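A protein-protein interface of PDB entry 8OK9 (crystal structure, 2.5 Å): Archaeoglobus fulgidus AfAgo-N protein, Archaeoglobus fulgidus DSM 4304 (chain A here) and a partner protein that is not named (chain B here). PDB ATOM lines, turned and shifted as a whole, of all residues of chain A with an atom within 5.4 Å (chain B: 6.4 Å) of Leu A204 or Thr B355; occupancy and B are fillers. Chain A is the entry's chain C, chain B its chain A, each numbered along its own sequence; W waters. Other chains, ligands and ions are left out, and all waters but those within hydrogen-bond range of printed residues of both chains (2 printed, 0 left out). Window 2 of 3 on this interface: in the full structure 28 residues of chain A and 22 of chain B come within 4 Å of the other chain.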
ATOM      1  N   TRP A 194       2.509 -24.148  17.083  1.00  0.00           N
ATOM      2  CA  TRP A 194       3.638 -23.419  16.515  1.00  0.00           C
ATOM      3  C   TRP A 194       4.538 -24.347  15.708  1.00  0.00           C
ATOM      4  O   TRP A 194       4.885 -24.049  14.561  1.00  0.00           O
ATOM      5  CB  TRP A 194       4.433 -22.727  17.624  1.00  0.00           C
ATOM      6  CG  TRP A 194       5.588 -21.929  17.104  1.00  0.00           C
ATOM      7  CD1 TRP A 194       5.571 -20.622  16.710  1.00  0.00           C
ATOM      8  CD2 TRP A 194       6.931 -22.389  16.907  1.00  0.00           C
ATOM      9  NE1 TRP A 194       6.819 -20.240  16.284  1.00  0.00           N
ATOM     10  CE2 TRP A 194       7.673 -21.306  16.395  1.00  0.00           C
ATOM     11  CE3 TRP A 194       7.578 -23.610  17.116  1.00  0.00           C
ATOM     12  CZ2 TRP A 194       9.027 -21.408  16.088  1.00  0.00           C
ATOM     13  CZ3 TRP A 194       8.924 -23.709  16.812  1.00  0.00           C
ATOM     14  CH2 TRP A 194       9.634 -22.614  16.304  1.00  0.00           C
ATOM     15  N   VAL A 195       4.913 -25.489  16.293  1.00  0.00           N
ATOM     16  CA  VAL A 195       5.772 -26.443  15.597  1.00  0.00           C
ATOM     17  C   VAL A 195       5.111 -26.921  14.309  1.00  0.00           C
ATOM     18  O   VAL A 195       5.776 -27.098  13.280  1.00  0.00           O
ATOM     19  CB  VAL A 195       6.121 -27.621  16.529  1.00  0.00           C
ATOM     20  CG1 VAL A 195       6.772 -28.756  15.751  1.00  0.00           C
ATOM     21  CG2 VAL A 195       7.029 -27.153  17.656  1.00  0.00           C
ATOM     22  N   GLN A 198       5.425 -24.283  11.614  1.00  0.00           N
ATOM     23  CA  GLN A 198       6.790 -24.287  11.098  1.00  0.00           C
ATOM     24  C   GLN A 198       7.041 -25.504  10.220  1.00  0.00           C
ATOM     25  O   GLN A 198       7.781 -25.424   9.233  1.00  0.00           O
ATOM     26  CB  GLN A 198       7.791 -24.238  12.252  1.00  0.00           C
ATOM     27  CG  GLN A 198       7.507 -23.135  13.256  1.00  0.00           C
ATOM     28  CD  GLN A 198       7.317 -21.781  12.603  1.00  0.00           C
ATOM     29  OE1 GLN A 198       8.027 -21.425  11.661  1.00  0.00           O
ATOM     30  NE2 GLN A 198       6.334 -21.029  13.083  1.00  0.00           N
ATOM     31  N   ALA A 199       6.425 -26.640  10.559  1.00  0.00           N
ATOM     32  CA  ALA A 199       6.550 -27.827   9.720  1.00  0.00           C
ATOM     33  C   ALA A 199       5.832 -27.634   8.391  1.00  0.00           C
ATOM     34  O   ALA A 199       6.376 -27.954   7.328  1.00  0.00           O
ATOM     35  CB  ALA A 199       6.006 -29.050  10.458  1.00  0.00           C
ATOM     36  N   ARG A 202       7.684 -25.754   6.155  1.00  0.00           N
ATOM     37  CA  ARG A 202       8.940 -26.437   5.847  1.00  0.00           C
ATOM     38  C   ARG A 202      10.149 -25.701   6.414  1.00  0.00           C
ATOM     39  O   ARG A 202      11.268 -25.857   5.913  1.00  0.00           O
ATOM     40  CB  ARG A 202       9.109 -26.662   4.338  1.00  0.00           C
ATOM     41  CG  ARG A 202       7.870 -27.219   3.654  1.00  0.00           C
ATOM     42  CD  ARG A 202       7.883 -28.740   3.631  1.00  0.00           C
ATOM     43  NE  ARG A 202       6.815 -29.282   2.796  1.00  0.00           N
ATOM     44  CZ  ARG A 202       5.554 -29.426   3.192  1.00  0.00           C
ATOM     45  NH1 ARG A 202       5.195 -29.069   4.418  1.00  0.00           N
ATOM     46  NH2 ARG A 202       4.650 -29.929   2.362  1.00  0.00           N
ATOM     47  N   HIS A 203       9.941 -24.895   7.458  1.00  0.00           N
ATOM     48  CA  HIS A 203      11.055 -24.277   8.164  1.00  0.00           C
ATOM     49  C   HIS A 203      11.696 -25.243   9.150  1.00  0.00           C
ATOM     50  O   HIS A 203      12.911 -25.183   9.375  1.00  0.00           O
ATOM     51  CB  HIS A 203      10.586 -23.021   8.902  1.00  0.00           C
ATOM     52  CG  HIS A 203      10.270 -21.870   7.999  1.00  0.00           C
ATOM     53  ND1 HIS A 203      10.230 -20.566   8.443  1.00  0.00           N
ATOM     54  CD2 HIS A 203       9.977 -21.827   6.678  1.00  0.00           C
ATOM     55  CE1 HIS A 203       9.928 -19.769   7.435  1.00  0.00           C
ATOM     56  NE2 HIS A 203       9.768 -20.509   6.353  1.00  0.00           N
ATOM     57  N   LEU A 204      10.899 -26.126   9.744  1.00  0.00           N
ATOM     58  CA  LEU A 204      11.378 -27.135  10.673  1.00  0.00           C
ATOM     59  C   LEU A 204      10.777 -28.480  10.294  1.00  0.00           C
ATOM     60  O   LEU A 204       9.811 -28.559   9.529  1.00  0.00           O
ATOM     61  CB  LEU A 204      11.010 -26.791  12.124  1.00  0.00           C
ATOM     62  CG  LEU A 204      11.638 -25.541  12.741  1.00  0.00           C
ATOM     63  CD1 LEU A 204      11.020 -25.250  14.100  1.00  0.00           C
ATOM     64  CD2 LEU A 204      13.143 -25.704  12.863  1.00  0.00           C
ATOM     65  N   THR A 205      11.363 -29.543  10.836  1.00  0.00           N
ATOM     66  CA  THR A 205      10.780 -30.861  10.689  1.00  0.00           C
ATOM     67  C   THR A 205       9.481 -30.938  11.487  1.00  0.00           C
ATOM     68  O   THR A 205       9.249 -30.128  12.387  1.00  0.00           O
ATOM     69  CB  THR A 205      11.757 -31.934  11.168  1.00  0.00           C
ATOM     70  OG1 THR A 205      12.140 -31.664  12.522  1.00  0.00           O
ATOM     71  CG2 THR A 205      12.999 -31.954  10.291  1.00  0.00           C
ATOM     72  N   PRO A 206       8.604 -31.902  11.165  1.00  0.00           N
ATOM     73  CA  PRO A 206       7.403 -32.108  11.988  1.00  0.00           C
ATOM     74  C   PRO A 206       7.740 -32.323  13.456  1.00  0.00           C
ATOM     75  O   PRO A 206       6.905 -32.091  14.337  1.00  0.00           O
ATOM     76  CB  PRO A 206       6.762 -33.352  11.365  1.00  0.00           C
ATOM     77  CG  PRO A 206       7.186 -33.305   9.940  1.00  0.00           C
ATOM     78  CD  PRO A 206       8.566 -32.701   9.926  1.00  0.00           C
ATOM     79  N   GLY A 208      10.021 -30.517  14.907  1.00  0.00           N
ATOM     80  CA  GLY A 208      10.433 -29.235  15.444  1.00  0.00           C
ATOM     81  C   GLY A 208      11.920 -28.988  15.397  1.00  0.00           C
ATOM     82  O   GLY A 208      12.436 -28.203  16.204  1.00  0.00           O
ATOM     83  N   LYS A 209      12.622 -29.631  14.467  1.00  0.00           N
ATOM     84  CA  LYS A 209      14.073 -29.657  14.417  1.00  0.00           C
ATOM     85  C   LYS A 209      14.559 -29.060  13.092  1.00  0.00           C
ATOM     86  O   LYS A 209      13.918 -29.214  12.041  1.00  0.00           O
ATOM     87  CB  LYS A 209      14.572 -31.108  14.590  1.00  0.00           C
ATOM     88  CG  LYS A 209      14.178 -31.756  15.927  1.00  0.00           C
ATOM     89  CD  LYS A 209      14.886 -31.007  17.033  1.00  0.00           C
ATOM     90  CE  LYS A 209      14.713 -31.657  18.377  1.00  0.00           C
ATOM     91  NZ  LYS A 209      13.310 -31.505  18.846  1.00  0.00           N
ATOM     92  N   LYS A 210      15.674 -28.328  13.148  1.00  0.00           N
ATOM     93  CA  LYS A 210      16.232 -27.744  11.935  1.00  0.00           C
ATOM     94  C   LYS A 210      16.876 -28.839  11.100  1.00  0.00           C
ATOM     95  O   LYS A 210      17.513 -29.750  11.636  1.00  0.00           O
ATOM     96  CB  LYS A 210      17.259 -26.649  12.249  1.00  0.00           C
ATOM     97  CG  LYS A 210      16.833 -25.626  13.296  1.00  0.00           C
ATOM     98  CD  LYS A 210      17.877 -24.525  13.458  1.00  0.00           C
ATOM     99  CE  LYS A 210      17.554 -23.652  14.659  1.00  0.00           C
ATOM    100  NZ  LYS A 210      18.645 -22.679  14.932  1.00  0.00           N
ATOM    101  N   TYR A 211      16.693 -28.762   9.783  1.00  0.00           N
ATOM    102  CA  TYR A 211      17.151 -29.822   8.893  1.00  0.00           C
ATOM    103  C   TYR A 211      17.844 -29.215   7.676  1.00  0.00           C
ATOM    104  O   TYR A 211      17.908 -27.993   7.509  1.00  0.00           O
ATOM    105  CB  TYR A 211      15.993 -30.752   8.498  1.00  0.00           C
ATOM    106  CG  TYR A 211      14.919 -30.127   7.635  1.00  0.00           C
ATOM    107  CD1 TYR A 211      14.065 -29.159   8.145  1.00  0.00           C
ATOM    108  CD2 TYR A 211      14.739 -30.533   6.319  1.00  0.00           C
ATOM    109  CE1 TYR A 211      13.079 -28.594   7.364  1.00  0.00           C
ATOM    110  CE2 TYR A 211      13.751 -29.974   5.529  1.00  0.00           C
ATOM    111  CZ  TYR A 211      12.923 -29.006   6.058  1.00  0.00           C
ATOM    112  OH  TYR A 211      11.940 -28.445   5.278  1.00  0.00           O
ATOM    113  N   ALA A 214      15.793 -27.292   4.160  1.00  0.00           N
ATOM    114  CA  ALA A 214      14.630 -26.469   4.485  1.00  0.00           C
ATOM    115  C   ALA A 214      14.318 -25.472   3.374  1.00  0.00           C
ATOM    116  O   ALA A 214      13.170 -25.363   2.928  1.00  0.00           O
ATOM    117  CB  ALA A 214      14.857 -25.744   5.811  1.00  0.00           C
ATOM    118  N   HIS B 323      21.267 -22.021   0.645  1.00  0.00           N
ATOM    119  CA  HIS B 323      21.235 -20.599   0.940  1.00  0.00           C
ATOM    120  C   HIS B 323      22.280 -19.856   0.115  1.00  0.00           C
ATOM    121  O   HIS B 323      23.337 -20.408  -0.207  1.00  0.00           O
ATOM    122  CB  HIS B 323      21.503 -20.332   2.426  1.00  0.00           C
ATOM    123  CG  HIS B 323      20.293 -20.473   3.296  1.00  0.00           C
ATOM    124  ND1 HIS B 323      19.669 -21.682   3.512  1.00  0.00           N
ATOM    125  CD2 HIS B 323      19.598 -19.558   4.011  1.00  0.00           C
ATOM    126  CE1 HIS B 323      18.640 -21.505   4.320  1.00  0.00           C
ATOM    127  NE2 HIS B 323      18.574 -20.225   4.637  1.00  0.00           N
ATOM    128  N   MET B 353      22.630 -26.269  10.798  1.00  0.00           N
ATOM    129  CA  MET B 353      21.299 -26.298  10.212  1.00  0.00           C
ATOM    130  C   MET B 353      20.582 -24.995  10.531  1.00  0.00           C
ATOM    131  O   MET B 353      20.635 -24.505  11.664  1.00  0.00           O
ATOM    132  CB  MET B 353      20.494 -27.484  10.744  1.00  0.00           C
ATOM    133  CG  MET B 353      21.188 -28.827  10.602  1.00  0.00           C
ATOM    134  SD  MET B 353      21.144 -29.443   8.911  1.00  0.00           S
ATOM    135  CE  MET B 353      21.428 -31.191   9.177  1.00  0.00           C
ATOM    136  N   VAL B 354      19.918 -24.428   9.527  1.00  0.00           N
ATOM    137  CA  VAL B 354      19.264 -23.136   9.673  1.00  0.00           C
ATOM    138  C   VAL B 354      17.822 -23.234   9.203  1.00  0.00           C
ATOM    139  O   VAL B 354      17.493 -23.990   8.284  1.00  0.00           O
ATOM    140  CB  VAL B 354      19.997 -22.025   8.888  1.00  0.00           C
ATOM    141  CG1 VAL B 354      21.356 -21.734   9.507  1.00  0.00           C
ATOM    142  CG2 VAL B 354      20.132 -22.408   7.419  1.00  0.00           C
ATOM    143  N   THR B 355      16.957 -22.465   9.855  1.00  0.00           N
ATOM    144  CA  THR B 355      15.683 -22.129   9.250  1.00  0.00           C
ATOM    145  C   THR B 355      15.931 -21.143   8.109  1.00  0.00           C
ATOM    146  O   THR B 355      16.921 -20.407   8.127  1.00  0.00           O
ATOM    147  CB  THR B 355      14.737 -21.521  10.283  1.00  0.00           C
ATOM    148  OG1 THR B 355      15.402 -20.461  10.980  1.00  0.00           O
ATOM    149  CG2 THR B 355      14.293 -22.578  11.284  1.00  0.00           C
ATOM    150  N   PRO B 356      15.072 -21.136   7.090  1.00  0.00           N
ATOM    151  CA  PRO B 356      15.301 -20.263   5.930  1.00  0.00           C
ATOM    152  C   PRO B 356      15.544 -18.813   6.328  1.00  0.00           C
ATOM    153  O   PRO B 356      14.819 -18.241   7.146  1.00  0.00           O
ATOM    154  CB  PRO B 356      14.012 -20.422   5.119  1.00  0.00           C
ATOM    155  CG  PRO B 356      13.573 -21.816   5.426  1.00  0.00           C
ATOM    156  CD  PRO B 356      13.931 -22.046   6.875  1.00  0.00           C
ATOM    157  N   ILE B 357      16.586 -18.222   5.743  1.00  0.00           N
ATOM    158  CA  ILE B 357      17.036 -16.876   6.079  1.00  0.00           C
ATOM    159  C   ILE B 357      16.585 -15.922   4.983  1.00  0.00           C
ATOM    160  O   ILE B 357      16.801 -16.183   3.793  1.00  0.00           O
ATOM    161  CB  ILE B 357      18.564 -16.830   6.250  1.00  0.00           C
ATOM    162  CG1 ILE B 357      19.011 -17.820   7.328  1.00  0.00           C
ATOM    163  CG2 ILE B 357      19.022 -15.418   6.594  1.00  0.00           C
ATOM    164  CD1 ILE B 357      20.505 -18.068   7.347  1.00  0.00           C
ATOM    165  N   LYS B 358      15.967 -14.812   5.383  1.00  0.00           N
ATOM    166  CA  LYS B 358      15.472 -13.846   4.412  1.00  0.00           C
ATOM    167  C   LYS B 358      16.490 -12.735   4.186  1.00  0.00           C
ATOM    168  O   LYS B 358      17.093 -12.242   5.145  1.00  0.00           O
ATOM    169  CB  LYS B 358      14.150 -13.236   4.886  1.00  0.00           C
ATOM    170  CG  LYS B 358      13.509 -12.281   3.889  1.00  0.00           C
ATOM    171  CD  LYS B 358      12.249 -11.649   4.452  1.00  0.00           C
ATOM    172  CE  LYS B 358      11.020 -12.455   4.074  1.00  0.00           C
ATOM    173  NZ  LYS B 358      10.762 -12.433   2.607  1.00  0.00           N
HETATM  174  O   HOH W   1      18.313 -20.915  11.966  1.00  0.00           O
HETATM  175  O   HOH W   2      18.791 -25.564   6.936  1.00  0.00           O
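The backbone carbonyl oxygen of Gln A198 is in hydrogen-bond range of the backbone NH of His A203 (2.8 Å). N of Leu A204 lies within hydrogen-bond range of O of Gln A198, 3.2 Å away. The side-chain hydroxyl of Tyr A211 is in hydrogen-bond range of the backbone carbonyl oxygen of Arg A202, at 2.7 Å.
CG2 of Thr B355 touches O of His A203, at 3.5 Å. His A203 touches Pro B356 (CD2 to CG, 3.8 Å). Thr B355 touches Leu A204 (CG2 to CD2, 3.7 Å). O of Met B353 touches CD of Lys A210 (3.3 Å). Tyr A211 touches Met B353 (C to SD, 3.5 Å). Ala A214 touches Pro B356.
Val A195 touches none of the printed residues of chain B. Gln A198 touches none of the printed residues of chain B. Of the printed residues of chain B, His A203 touches Thr B355 and Pro B356. Of chain B, only Thr B355 (3.7 Å) comes within 4 Å of Leu A204. Printed residues of chain B within 4 Å of Lys A210: Met B353. Of the printed residues of chain B, Tyr A211 touches Met B353. Of the printed residues of chain B, Ala A214 touches Pro B356. Of the printed residues of chain A, Met B353 touches Lys A210 and Tyr A211. Of the printed residues of chain A, Thr B355 touches His A203 (3.5 Å) and Leu A204 (3.7 Å).
Of the 14 printed residues of chain A, 5 touch a printed residue of chain B. Hydrophobic or aromatic side chains of chain A within 4 Å of the printed part of chain B: His A203, Leu A204 and Ala A214. Along chain A the printed residues that touch a printed residue of chain B span positions 203 to 214. Printed residues of chain B that touch a printed residue of chain A: Met B353, Thr B355 and Pro B356. Among the printed residues, no Asp or Glu carboxylate lies within 4 Å of a Lys or Arg side-chain nitrogen of the other chain.
Water W2 lies within hydrogen-bond range of O of Val B354 (2.4 Å) and O of Tyr A211 (2.6 Å). Water W1 bridges N of Thr B355 (2.9 Å) and NZ of Lys A210 (3.5 Å).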
